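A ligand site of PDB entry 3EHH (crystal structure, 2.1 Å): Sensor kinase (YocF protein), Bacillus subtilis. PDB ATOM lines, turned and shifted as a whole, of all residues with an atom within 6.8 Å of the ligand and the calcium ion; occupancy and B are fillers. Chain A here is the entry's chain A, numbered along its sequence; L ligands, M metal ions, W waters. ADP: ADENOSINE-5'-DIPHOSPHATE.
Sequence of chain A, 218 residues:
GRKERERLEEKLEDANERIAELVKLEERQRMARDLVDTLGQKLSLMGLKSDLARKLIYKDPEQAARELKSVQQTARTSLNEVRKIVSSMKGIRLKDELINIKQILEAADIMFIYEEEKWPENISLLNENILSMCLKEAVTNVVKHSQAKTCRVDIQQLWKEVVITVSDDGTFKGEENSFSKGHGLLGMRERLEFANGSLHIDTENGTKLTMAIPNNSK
Val 142 touches the ligand. Ser 146 touches the ligand. Thr 171 touches the ligand (O to C2, 3.3 Å). Phe 172 touches the ligand. Thr 207 touches the ligand. Hydrophobic or aromatic side chains within 4 Å of the ligand: His 145, Phe 172 and Leu 185. Within 4 Å of the ligand: Glu 137, Asn 141, Val 142, His 145, Ser 146, Asp 168, Thr 171, Phe 172, Lys 173, Gly 174, Gly 184, Leu 185 and Thr 207. The nearest printed residue that does not touch the ligand is His 183 (4.1 Å).
Water W1 lies within hydrogen-bond range of O2B of the ligand (2.8 Å) and N of Gly 184 (2.9 Å). Water W2 lies within hydrogen-bond range of N7 of the ligand (2.8 Å) and ND2 of Asn 141 (2.9 Å). Water W5 lies within hydrogen-bond range of OG1 of Thr 207 (2.6 Å), OD1 of Asp 168 (2.7 Å), N1 of the ligand (2.9 Å) and N of Thr 171 (3.4 Å). Water W4 bridges O of Ala 138 (2.6 Å) and N6 of the ligand (3.0 Å).
O1A of the ligand is in hydrogen-bond range of N of Gly 184, 3.2 Å away. N of Leu 185 is in hydrogen-bond range of O1A of the ligand, at 2.8 Å. O3B of the ligand sits close to NE2 of His 145. The backbone NH (N) of Gly 174 lies within hydrogen-bond range of an oxygen (O2') of the ligand (3.3 Å). N of Lys 173 lies within hydrogen-bond range of N3 of the ligand (3.1 Å). A nitrogen (N6) of the ligand is in hydrogen-bond range of the side-chain carboxylate of Asp 168 (3.1 Å).
The calcium ion is bound by O2A of the ligand (2.2 Å). The side-chain amide oxygen (OD1) of Asn 141 binds the calcium ion. The calcium ion is bound by OE2 of Glu 137 (2.3 Å). The calcium ion is bound by water W3, at 2.3 Å. Water W1 binds the calcium ion, at 2.3 Å. An oxygen (O3B) of the ligand binds the calcium ion, at 2.4 Å. The calcium ion has six donor atoms within binding distance.
O of Thr 171 sits at hydrogen-bond distance from NZ of Lys 173 (2.6 Å). The side-chain carboxylate (OD1) of Asp 168 sits at hydrogen-bond distance from the backbone NH (N) of Gly 170, 2.8 Å away. O of Thr 207 sits at hydrogen-bond distance from N of Asp 168, at 2.9 Å. The backbone NH of Thr 171 is in hydrogen-bond range of the backbone carbonyl oxygen of Ser 146 (3.1 Å). NZ of Lys 173 lies within hydrogen-bond range of O of His 145 (3.0 Å). The backbone carbonyl oxygen of Val 142 sits at hydrogen-bond distance from the side-chain hydroxyl of Ser 146, 2.5 Å away. O of Ser 146 lies within hydrogen-bond range of NZ of Lys 173, 3.2 Å away. The side-chain amino group (NZ) of Lys 173 sits at hydrogen-bond distance from the side-chain amide oxygen (OE1) of Gln 147 (2.8 Å).
The nearest printed residue that does not touch the calcium ion is His 145 (4.2 Å).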
ATOM      1  N   GLU A 137      -1.674  -0.362  -7.387  1.00  0.00           N
ATOM      2  CA  GLU A 137      -0.256  -0.317  -7.719  1.00  0.00           C
ATOM      3  C   GLU A 137       0.592   0.054  -6.496  1.00  0.00           C
ATOM      4  O   GLU A 137       1.654  -0.510  -6.313  1.00  0.00           O
ATOM      5  CB  GLU A 137       0.010   0.661  -8.853  1.00  0.00           C
ATOM      6  CG  GLU A 137       1.475   0.794  -9.221  1.00  0.00           C
ATOM      7  CD  GLU A 137       2.135  -0.542  -9.701  1.00  0.00           C
ATOM      8  OE1 GLU A 137       1.419  -1.467 -10.139  1.00  0.00           O
ATOM      9  OE2 GLU A 137       3.362  -0.645  -9.641  1.00  0.00           O
ATOM     10  N   ALA A 138       0.121   1.016  -5.682  1.00  0.00           N
ATOM     11  CA  ALA A 138       0.811   1.458  -4.449  1.00  0.00           C
ATOM     12  C   ALA A 138       1.065   0.304  -3.454  1.00  0.00           C
ATOM     13  O   ALA A 138       2.155   0.163  -2.920  1.00  0.00           O
ATOM     14  CB  ALA A 138       0.015   2.632  -3.724  1.00  0.00           C
ATOM     15  N   VAL A 139       0.026  -0.481  -3.203  1.00  0.00           N
ATOM     16  CA  VAL A 139       0.124  -1.626  -2.314  1.00  0.00           C
ATOM     17  C   VAL A 139       0.941  -2.784  -2.879  1.00  0.00           C
ATOM     18  O   VAL A 139       1.767  -3.378  -2.156  1.00  0.00           O
ATOM     19  CB  VAL A 139      -1.292  -2.070  -1.901  1.00  0.00           C
ATOM     20  CG1 VAL A 139      -1.226  -3.349  -1.066  1.00  0.00           C
ATOM     21  CG2 VAL A 139      -1.988  -0.906  -1.193  1.00  0.00           C
ATOM     22  N   THR A 140       0.791  -3.056  -4.175  1.00  0.00           N
ATOM     23  CA  THR A 140       1.658  -3.997  -4.877  1.00  0.00           C
ATOM     24  C   THR A 140       3.128  -3.611  -4.691  1.00  0.00           C
ATOM     25  O   THR A 140       3.943  -4.448  -4.395  1.00  0.00           O
ATOM     26  CB  THR A 140       1.290  -4.076  -6.382  1.00  0.00           C
ATOM     27  OG1 THR A 140      -0.097  -4.381  -6.478  1.00  0.00           O
ATOM     28  CG2 THR A 140       2.102  -5.099  -7.125  1.00  0.00           C
ATOM     29  N   ASN A 141       3.435  -2.325  -4.810  1.00  0.00           N
ATOM     30  CA  ASN A 141       4.791  -1.895  -4.631  1.00  0.00           C
ATOM     31  C   ASN A 141       5.230  -2.097  -3.174  1.00  0.00           C
ATOM     32  O   ASN A 141       6.371  -2.429  -2.932  1.00  0.00           O
ATOM     33  CB  ASN A 141       4.957  -0.431  -5.020  1.00  0.00           C
ATOM     34  CG  ASN A 141       5.176  -0.236  -6.501  1.00  0.00           C
ATOM     35  OD1 ASN A 141       5.399  -1.181  -7.244  1.00  0.00           O
ATOM     36  ND2 ASN A 141       5.071   1.008  -6.936  1.00  0.00           N
ATOM     37  N   VAL A 142       4.311  -1.893  -2.218  1.00  0.00           N
ATOM     38  CA  VAL A 142       4.610  -2.150  -0.811  1.00  0.00           C
ATOM     39  C   VAL A 142       5.015  -3.626  -0.625  1.00  0.00           C
ATOM     40  O   VAL A 142       5.983  -3.939   0.063  1.00  0.00           O
ATOM     41  CB  VAL A 142       3.390  -1.769   0.116  1.00  0.00           C
ATOM     42  CG1 VAL A 142       3.603  -2.294   1.575  1.00  0.00           C
ATOM     43  CG2 VAL A 142       3.147  -0.262   0.155  1.00  0.00           C
ATOM     44  N   VAL A 143       4.262  -4.516  -1.271  1.00  0.00           N
ATOM     45  CA  VAL A 143       4.489  -5.915  -1.128  1.00  0.00           C
ATOM     46  C   VAL A 143       5.760  -6.314  -1.848  1.00  0.00           C
ATOM     47  O   VAL A 143       6.526  -7.070  -1.294  1.00  0.00           O
ATOM     48  CB  VAL A 143       3.318  -6.735  -1.668  1.00  0.00           C
ATOM     49  CG1 VAL A 143       3.708  -8.243  -1.777  1.00  0.00           C
ATOM     50  CG2 VAL A 143       2.101  -6.532  -0.825  1.00  0.00           C
ATOM     51  N   LYS A 144       5.995  -5.839  -3.061  1.00  0.00           N
ATOM     52  CA  LYS A 144       7.176  -6.304  -3.784  1.00  0.00           C
ATOM     53  C   LYS A 144       8.477  -5.601  -3.369  1.00  0.00           C
ATOM     54  O   LYS A 144       9.523  -6.168  -3.513  1.00  0.00           O
ATOM     55  CB  LYS A 144       6.952  -6.201  -5.292  1.00  0.00           C
ATOM     56  CG  LYS A 144       5.644  -6.933  -5.736  1.00  0.00           C
ATOM     57  CD  LYS A 144       5.564  -7.236  -7.229  1.00  0.00           C
ATOM     58  CE  LYS A 144       4.515  -8.339  -7.512  1.00  0.00           C
ATOM     59  NZ  LYS A 144       3.638  -8.093  -8.712  1.00  0.00           N
ATOM     60  N   HIS A 145       8.428  -4.360  -2.878  1.00  0.00           N
ATOM     61  CA  HIS A 145       9.669  -3.580  -2.747  1.00  0.00           C
ATOM     62  C   HIS A 145      10.042  -3.124  -1.344  1.00  0.00           C
ATOM     63  O   HIS A 145      11.213  -2.924  -1.080  1.00  0.00           O
ATOM     64  CB  HIS A 145       9.618  -2.346  -3.648  1.00  0.00           C
ATOM     65  CG  HIS A 145       9.412  -2.671  -5.091  1.00  0.00           C
ATOM     66  ND1 HIS A 145      10.221  -3.538  -5.784  1.00  0.00           N
ATOM     67  CD2 HIS A 145       8.483  -2.239  -5.982  1.00  0.00           C
ATOM     68  CE1 HIS A 145       9.812  -3.633  -7.035  1.00  0.00           C
ATOM     69  NE2 HIS A 145       8.759  -2.854  -7.183  1.00  0.00           N
ATOM     70  N   SER A 146       9.058  -2.875  -0.481  1.00  0.00           N
ATOM     71  CA  SER A 146       9.322  -2.102   0.738  1.00  0.00           C
ATOM     72  C   SER A 146      10.042  -2.870   1.835  1.00  0.00           C
ATOM     73  O   SER A 146      10.817  -2.282   2.567  1.00  0.00           O
ATOM     74  CB  SER A 146       8.018  -1.546   1.312  1.00  0.00           C
ATOM     75  OG  SER A 146       7.205  -2.571   1.817  1.00  0.00           O
ATOM     76  N   GLN A 147       9.756  -4.166   1.925  1.00  0.00           N
ATOM     77  CA  GLN A 147      10.025  -4.976   3.131  1.00  0.00           C
ATOM     78  C   GLN A 147       9.381  -4.359   4.400  1.00  0.00           C
ATOM     79  O   GLN A 147       9.907  -4.468   5.477  1.00  0.00           O
ATOM     80  CB  GLN A 147      11.518  -5.218   3.314  1.00  0.00           C
ATOM     81  CG  GLN A 147      12.171  -5.928   2.147  1.00  0.00           C
ATOM     82  CD  GLN A 147      13.647  -5.579   2.042  1.00  0.00           C
ATOM     83  OE1 GLN A 147      13.992  -4.451   1.681  1.00  0.00           O
ATOM     84  NE2 GLN A 147      14.521  -6.508   2.378  1.00  0.00           N
ATOM     85  N   ASP A 168       4.010   3.077   4.154  1.00  0.00           N
ATOM     86  CA  ASP A 168       4.588   1.878   4.672  1.00  0.00           C
ATOM     87  C   ASP A 168       5.815   2.241   5.468  1.00  0.00           C
ATOM     88  O   ASP A 168       6.381   3.336   5.337  1.00  0.00           O
ATOM     89  CB  ASP A 168       4.896   0.853   3.560  1.00  0.00           C
ATOM     90  CG  ASP A 168       6.061   1.278   2.671  1.00  0.00           C
ATOM     91  OD1 ASP A 168       7.193   1.405   3.204  1.00  0.00           O
ATOM     92  OD2 ASP A 168       5.829   1.477   1.438  1.00  0.00           O
ATOM     93  N   GLY A 170       8.695   0.464   5.425  1.00  0.00           N
ATOM     94  CA  GLY A 170       9.868  -0.199   4.862  1.00  0.00           C
ATOM     95  C   GLY A 170      10.851   0.846   4.430  1.00  0.00           C
ATOM     96  O   GLY A 170      10.848   1.926   4.960  1.00  0.00           O
ATOM     97  N   THR A 171      11.708   0.538   3.461  1.00  0.00           N
ATOM     98  CA  THR A 171      12.677   1.520   2.963  1.00  0.00           C
ATOM     99  C   THR A 171      12.580   1.615   1.438  1.00  0.00           C
ATOM    100  O   THR A 171      12.488   0.599   0.742  1.00  0.00           O
ATOM    101  CB  THR A 171      14.091   1.123   3.374  1.00  0.00           C
ATOM    102  OG1 THR A 171      14.361  -0.193   2.901  1.00  0.00           O
ATOM    103  CG2 THR A 171      14.235   1.133   4.888  1.00  0.00           C
ATOM    104  N   PHE A 172      12.610   2.841   0.908  1.00  0.00           N
ATOM    105  CA  PHE A 172      12.468   3.061  -0.534  1.00  0.00           C
ATOM    106  C   PHE A 172      13.711   2.627  -1.302  1.00  0.00           C
ATOM    107  O   PHE A 172      14.822   2.985  -0.930  1.00  0.00           O
ATOM    108  CB  PHE A 172      12.189   4.530  -0.834  1.00  0.00           C
ATOM    109  CG  PHE A 172      11.812   4.785  -2.254  1.00  0.00           C
ATOM    110  CD1 PHE A 172      10.537   4.470  -2.718  1.00  0.00           C
ATOM    111  CD2 PHE A 172      12.734   5.332  -3.132  1.00  0.00           C
ATOM    112  CE1 PHE A 172      10.190   4.695  -4.032  1.00  0.00           C
ATOM    113  CE2 PHE A 172      12.380   5.563  -4.450  1.00  0.00           C
ATOM    114  CZ  PHE A 172      11.105   5.236  -4.906  1.00  0.00           C
ATOM    115  N   LYS A 173      13.511   1.877  -2.379  1.00  0.00           N
ATOM    116  CA  LYS A 173      14.597   1.236  -3.079  1.00  0.00           C
ATOM    117  C   LYS A 173      15.094   1.978  -4.316  1.00  0.00           C
ATOM    118  O   LYS A 173      16.228   1.774  -4.734  1.00  0.00           O
ATOM    119  CB  LYS A 173      14.185  -0.197  -3.431  1.00  0.00           C
ATOM    120  CG  LYS A 173      13.754  -1.012  -2.191  1.00  0.00           C
ATOM    121  CD  LYS A 173      14.850  -0.997  -1.096  1.00  0.00           C
ATOM    122  CE  LYS A 173      14.621  -2.043  -0.024  1.00  0.00           C
ATOM    123  NZ  LYS A 173      13.327  -1.869   0.693  1.00  0.00           N
ATOM    124  N   GLY A 174      14.269   2.859  -4.884  1.00  0.00           N
ATOM    125  CA  GLY A 174      14.625   3.581  -6.120  1.00  0.00           C
ATOM    126  C   GLY A 174      16.033   4.159  -6.127  1.00  0.00           C
ATOM    127  O   GLY A 174      16.232   5.315  -5.781  1.00  0.00           O
ATOM    128  N   HIS A 183       7.293   1.618 -15.306  1.00  0.00           N
ATOM    129  CA  HIS A 183       6.024   0.920 -15.166  1.00  0.00           C
ATOM    130  C   HIS A 183       5.092   1.661 -14.229  1.00  0.00           C
ATOM    131  O   HIS A 183       4.380   2.595 -14.627  1.00  0.00           O
ATOM    132  N   GLY A 184       5.139   1.267 -12.960  1.00  0.00           N
ATOM    133  CA  GLY A 184       4.152   1.653 -11.973  1.00  0.00           C
ATOM    134  C   GLY A 184       4.018   3.136 -11.638  1.00  0.00           C
ATOM    135  O   GLY A 184       2.936   3.682 -11.759  1.00  0.00           O
ATOM    136  N   LEU A 185       5.109   3.759 -11.206  1.00  0.00           N
ATOM    137  CA  LEU A 185       5.051   5.109 -10.644  1.00  0.00           C
ATOM    138  C   LEU A 185       4.685   6.179 -11.679  1.00  0.00           C
ATOM    139  O   LEU A 185       3.921   7.122 -11.365  1.00  0.00           O
ATOM    140  CB  LEU A 185       6.362   5.463  -9.938  1.00  0.00           C
ATOM    141  CG  LEU A 185       6.558   4.800  -8.567  1.00  0.00           C
ATOM    142  CD1 LEU A 185       8.005   5.038  -8.047  1.00  0.00           C
ATOM    143  CD2 LEU A 185       5.499   5.276  -7.546  1.00  0.00           C
ATOM    144  N   LEU A 186       5.218   6.044 -12.892  1.00  0.00           N
ATOM    145  CA  LEU A 186       4.870   6.966 -13.970  1.00  0.00           C
ATOM    146  C   LEU A 186       3.445   6.665 -14.470  1.00  0.00           C
ATOM    147  O   LEU A 186       2.678   7.578 -14.720  1.00  0.00           O
ATOM    148  CB  LEU A 186       5.917   6.941 -15.084  1.00  0.00           C
ATOM    149  CG  LEU A 186       6.347   8.264 -15.775  1.00  0.00           C
ATOM    150  CD1 LEU A 186       6.147   8.230 -17.296  1.00  0.00           C
ATOM    151  CD2 LEU A 186       5.683   9.523 -15.168  1.00  0.00           C
ATOM    152  N   GLY A 187       3.066   5.392 -14.579  1.00  0.00           N
ATOM    153  CA  GLY A 187       1.672   5.037 -14.859  1.00  0.00           C
ATOM    154  C   GLY A 187       0.700   5.724 -13.898  1.00  0.00           C
ATOM    155  O   GLY A 187      -0.349   6.251 -14.310  1.00  0.00           O
ATOM    156  N   MET A 188       1.041   5.724 -12.606  1.00  0.00           N
ATOM    157  CA  MET A 188       0.225   6.357 -11.581  1.00  0.00           C
ATOM    158  C   MET A 188       0.165   7.865 -11.797  1.00  0.00           C
ATOM    159  O   MET A 188      -0.917   8.421 -11.755  1.00  0.00           O
ATOM    160  CB  MET A 188       0.780   6.037 -10.176  1.00  0.00           C
ATOM    161  CG  MET A 188       0.586   4.583  -9.721  1.00  0.00           C
ATOM    162  SD  MET A 188       1.177   4.346  -7.837  1.00  0.00           S
ATOM    163  CE  MET A 188       0.964   6.229  -7.317  1.00  0.00           C
ATOM    164  N   THR A 207       7.968   4.881   2.926  1.00  0.00           N
ATOM    165  CA  THR A 207       7.422   5.458   1.695  1.00  0.00           C
ATOM    166  C   THR A 207       5.956   5.870   1.905  1.00  0.00           C
ATOM    167  O   THR A 207       5.130   5.043   2.286  1.00  0.00           O
ATOM    168  CB  THR A 207       7.496   4.439   0.540  1.00  0.00           C
ATOM    169  OG1 THR A 207       8.844   3.972   0.391  1.00  0.00           O
ATOM    170  CG2 THR A 207       7.006   5.048  -0.773  1.00  0.00           C
ATOM    171  N   LEU A 209       2.893   7.563  -0.305  1.00  0.00           N
ATOM    172  CA  LEU A 209       2.293   8.058  -1.553  1.00  0.00           C
ATOM    173  C   LEU A 209       1.032   8.780  -1.202  1.00  0.00           C
ATOM    174  O   LEU A 209       0.166   8.197  -0.602  1.00  0.00           O
ATOM    175  CB  LEU A 209       1.912   6.898  -2.482  1.00  0.00           C
ATOM    176  CG  LEU A 209       2.941   6.497  -3.543  1.00  0.00           C
ATOM    177  CD1 LEU A 209       4.246   6.227  -2.905  1.00  0.00           C
ATOM    178  CD2 LEU A 209       2.427   5.309  -4.393  1.00  0.00           C
HETATM  179  PB  ADP L   1       8.719  -1.609 -10.705  1.00  0.00           P
HETATM  180  O1B ADP L   1      10.174  -1.410 -10.329  1.00  0.00           O
HETATM  181  O2B ADP L   1       8.380  -2.256 -11.988  1.00  0.00           O
HETATM  182  O3B ADP L   1       7.783  -2.095  -9.614  1.00  0.00           O
HETATM  183  PA  ADP L   1       7.624   1.026 -10.154  1.00  0.00           P
HETATM  184  O1A ADP L   1       7.482   2.285 -10.952  1.00  0.00           O
HETATM  185  O2A ADP L   1       6.356   0.422  -9.581  1.00  0.00           O
HETATM  186  O3A ADP L   1       8.388  -0.060 -11.049  1.00  0.00           O
HETATM  187  O5' ADP L   1       8.599   1.389  -8.973  1.00  0.00           O
HETATM  188  C5' ADP L   1       9.834   2.001  -9.322  1.00  0.00           C
HETATM  189  C4' ADP L   1      10.868   1.663  -8.263  1.00  0.00           C
HETATM  190  O4' ADP L   1      10.683   2.541  -7.158  1.00  0.00           O
HETATM  191  C3' ADP L   1      10.729   0.273  -7.669  1.00  0.00           C
HETATM  192  O3' ADP L   1      11.408  -0.742  -8.382  1.00  0.00           O
HETATM  193  C2' ADP L   1      11.356   0.452  -6.315  1.00  0.00           C
HETATM  194  O2' ADP L   1      12.770   0.455  -6.497  1.00  0.00           O
HETATM  195  C1' ADP L   1      10.900   1.846  -5.922  1.00  0.00           C
HETATM  196  N9  ADP L   1       9.662   1.743  -5.122  1.00  0.00           N
HETATM  197  C8  ADP L   1       8.409   1.988  -5.536  1.00  0.00           C
HETATM  198  N7  ADP L   1       7.522   1.770  -4.532  1.00  0.00           N
HETATM  199  C5  ADP L   1       8.203   1.405  -3.446  1.00  0.00           C
HETATM  200  C6  ADP L   1       7.910   1.041  -2.044  1.00  0.00           C
HETATM  201  N6  ADP L   1       6.662   1.022  -1.558  1.00  0.00           N
HETATM  202  N1  ADP L   1       8.942   0.717  -1.238  1.00  0.00           N
HETATM  203  C2  ADP L   1      10.198   0.719  -1.687  1.00  0.00           C
HETATM  204  N3  ADP L   1      10.550   1.048  -2.943  1.00  0.00           N
HETATM  205  C4  ADP L   1       9.623   1.398  -3.852  1.00  0.00           C
HETATM  206 CA    CA M   1       5.438  -1.600  -9.494  1.00  0.00          CA
HETATM  207  O   HOH W   1       5.804  -1.271 -11.759  1.00  0.00           O
HETATM  208  O   HOH W   2       4.973   2.951  -4.779  1.00  0.00           O
HETATM  209  O   HOH W   3       4.232  -3.527  -9.781  1.00  0.00           O
HETATM  210  O   HOH W   4       3.957   2.011  -2.525  1.00  0.00           O
HETATM  211  O   HOH W   5       9.205   1.665   1.441  1.00  0.00           O
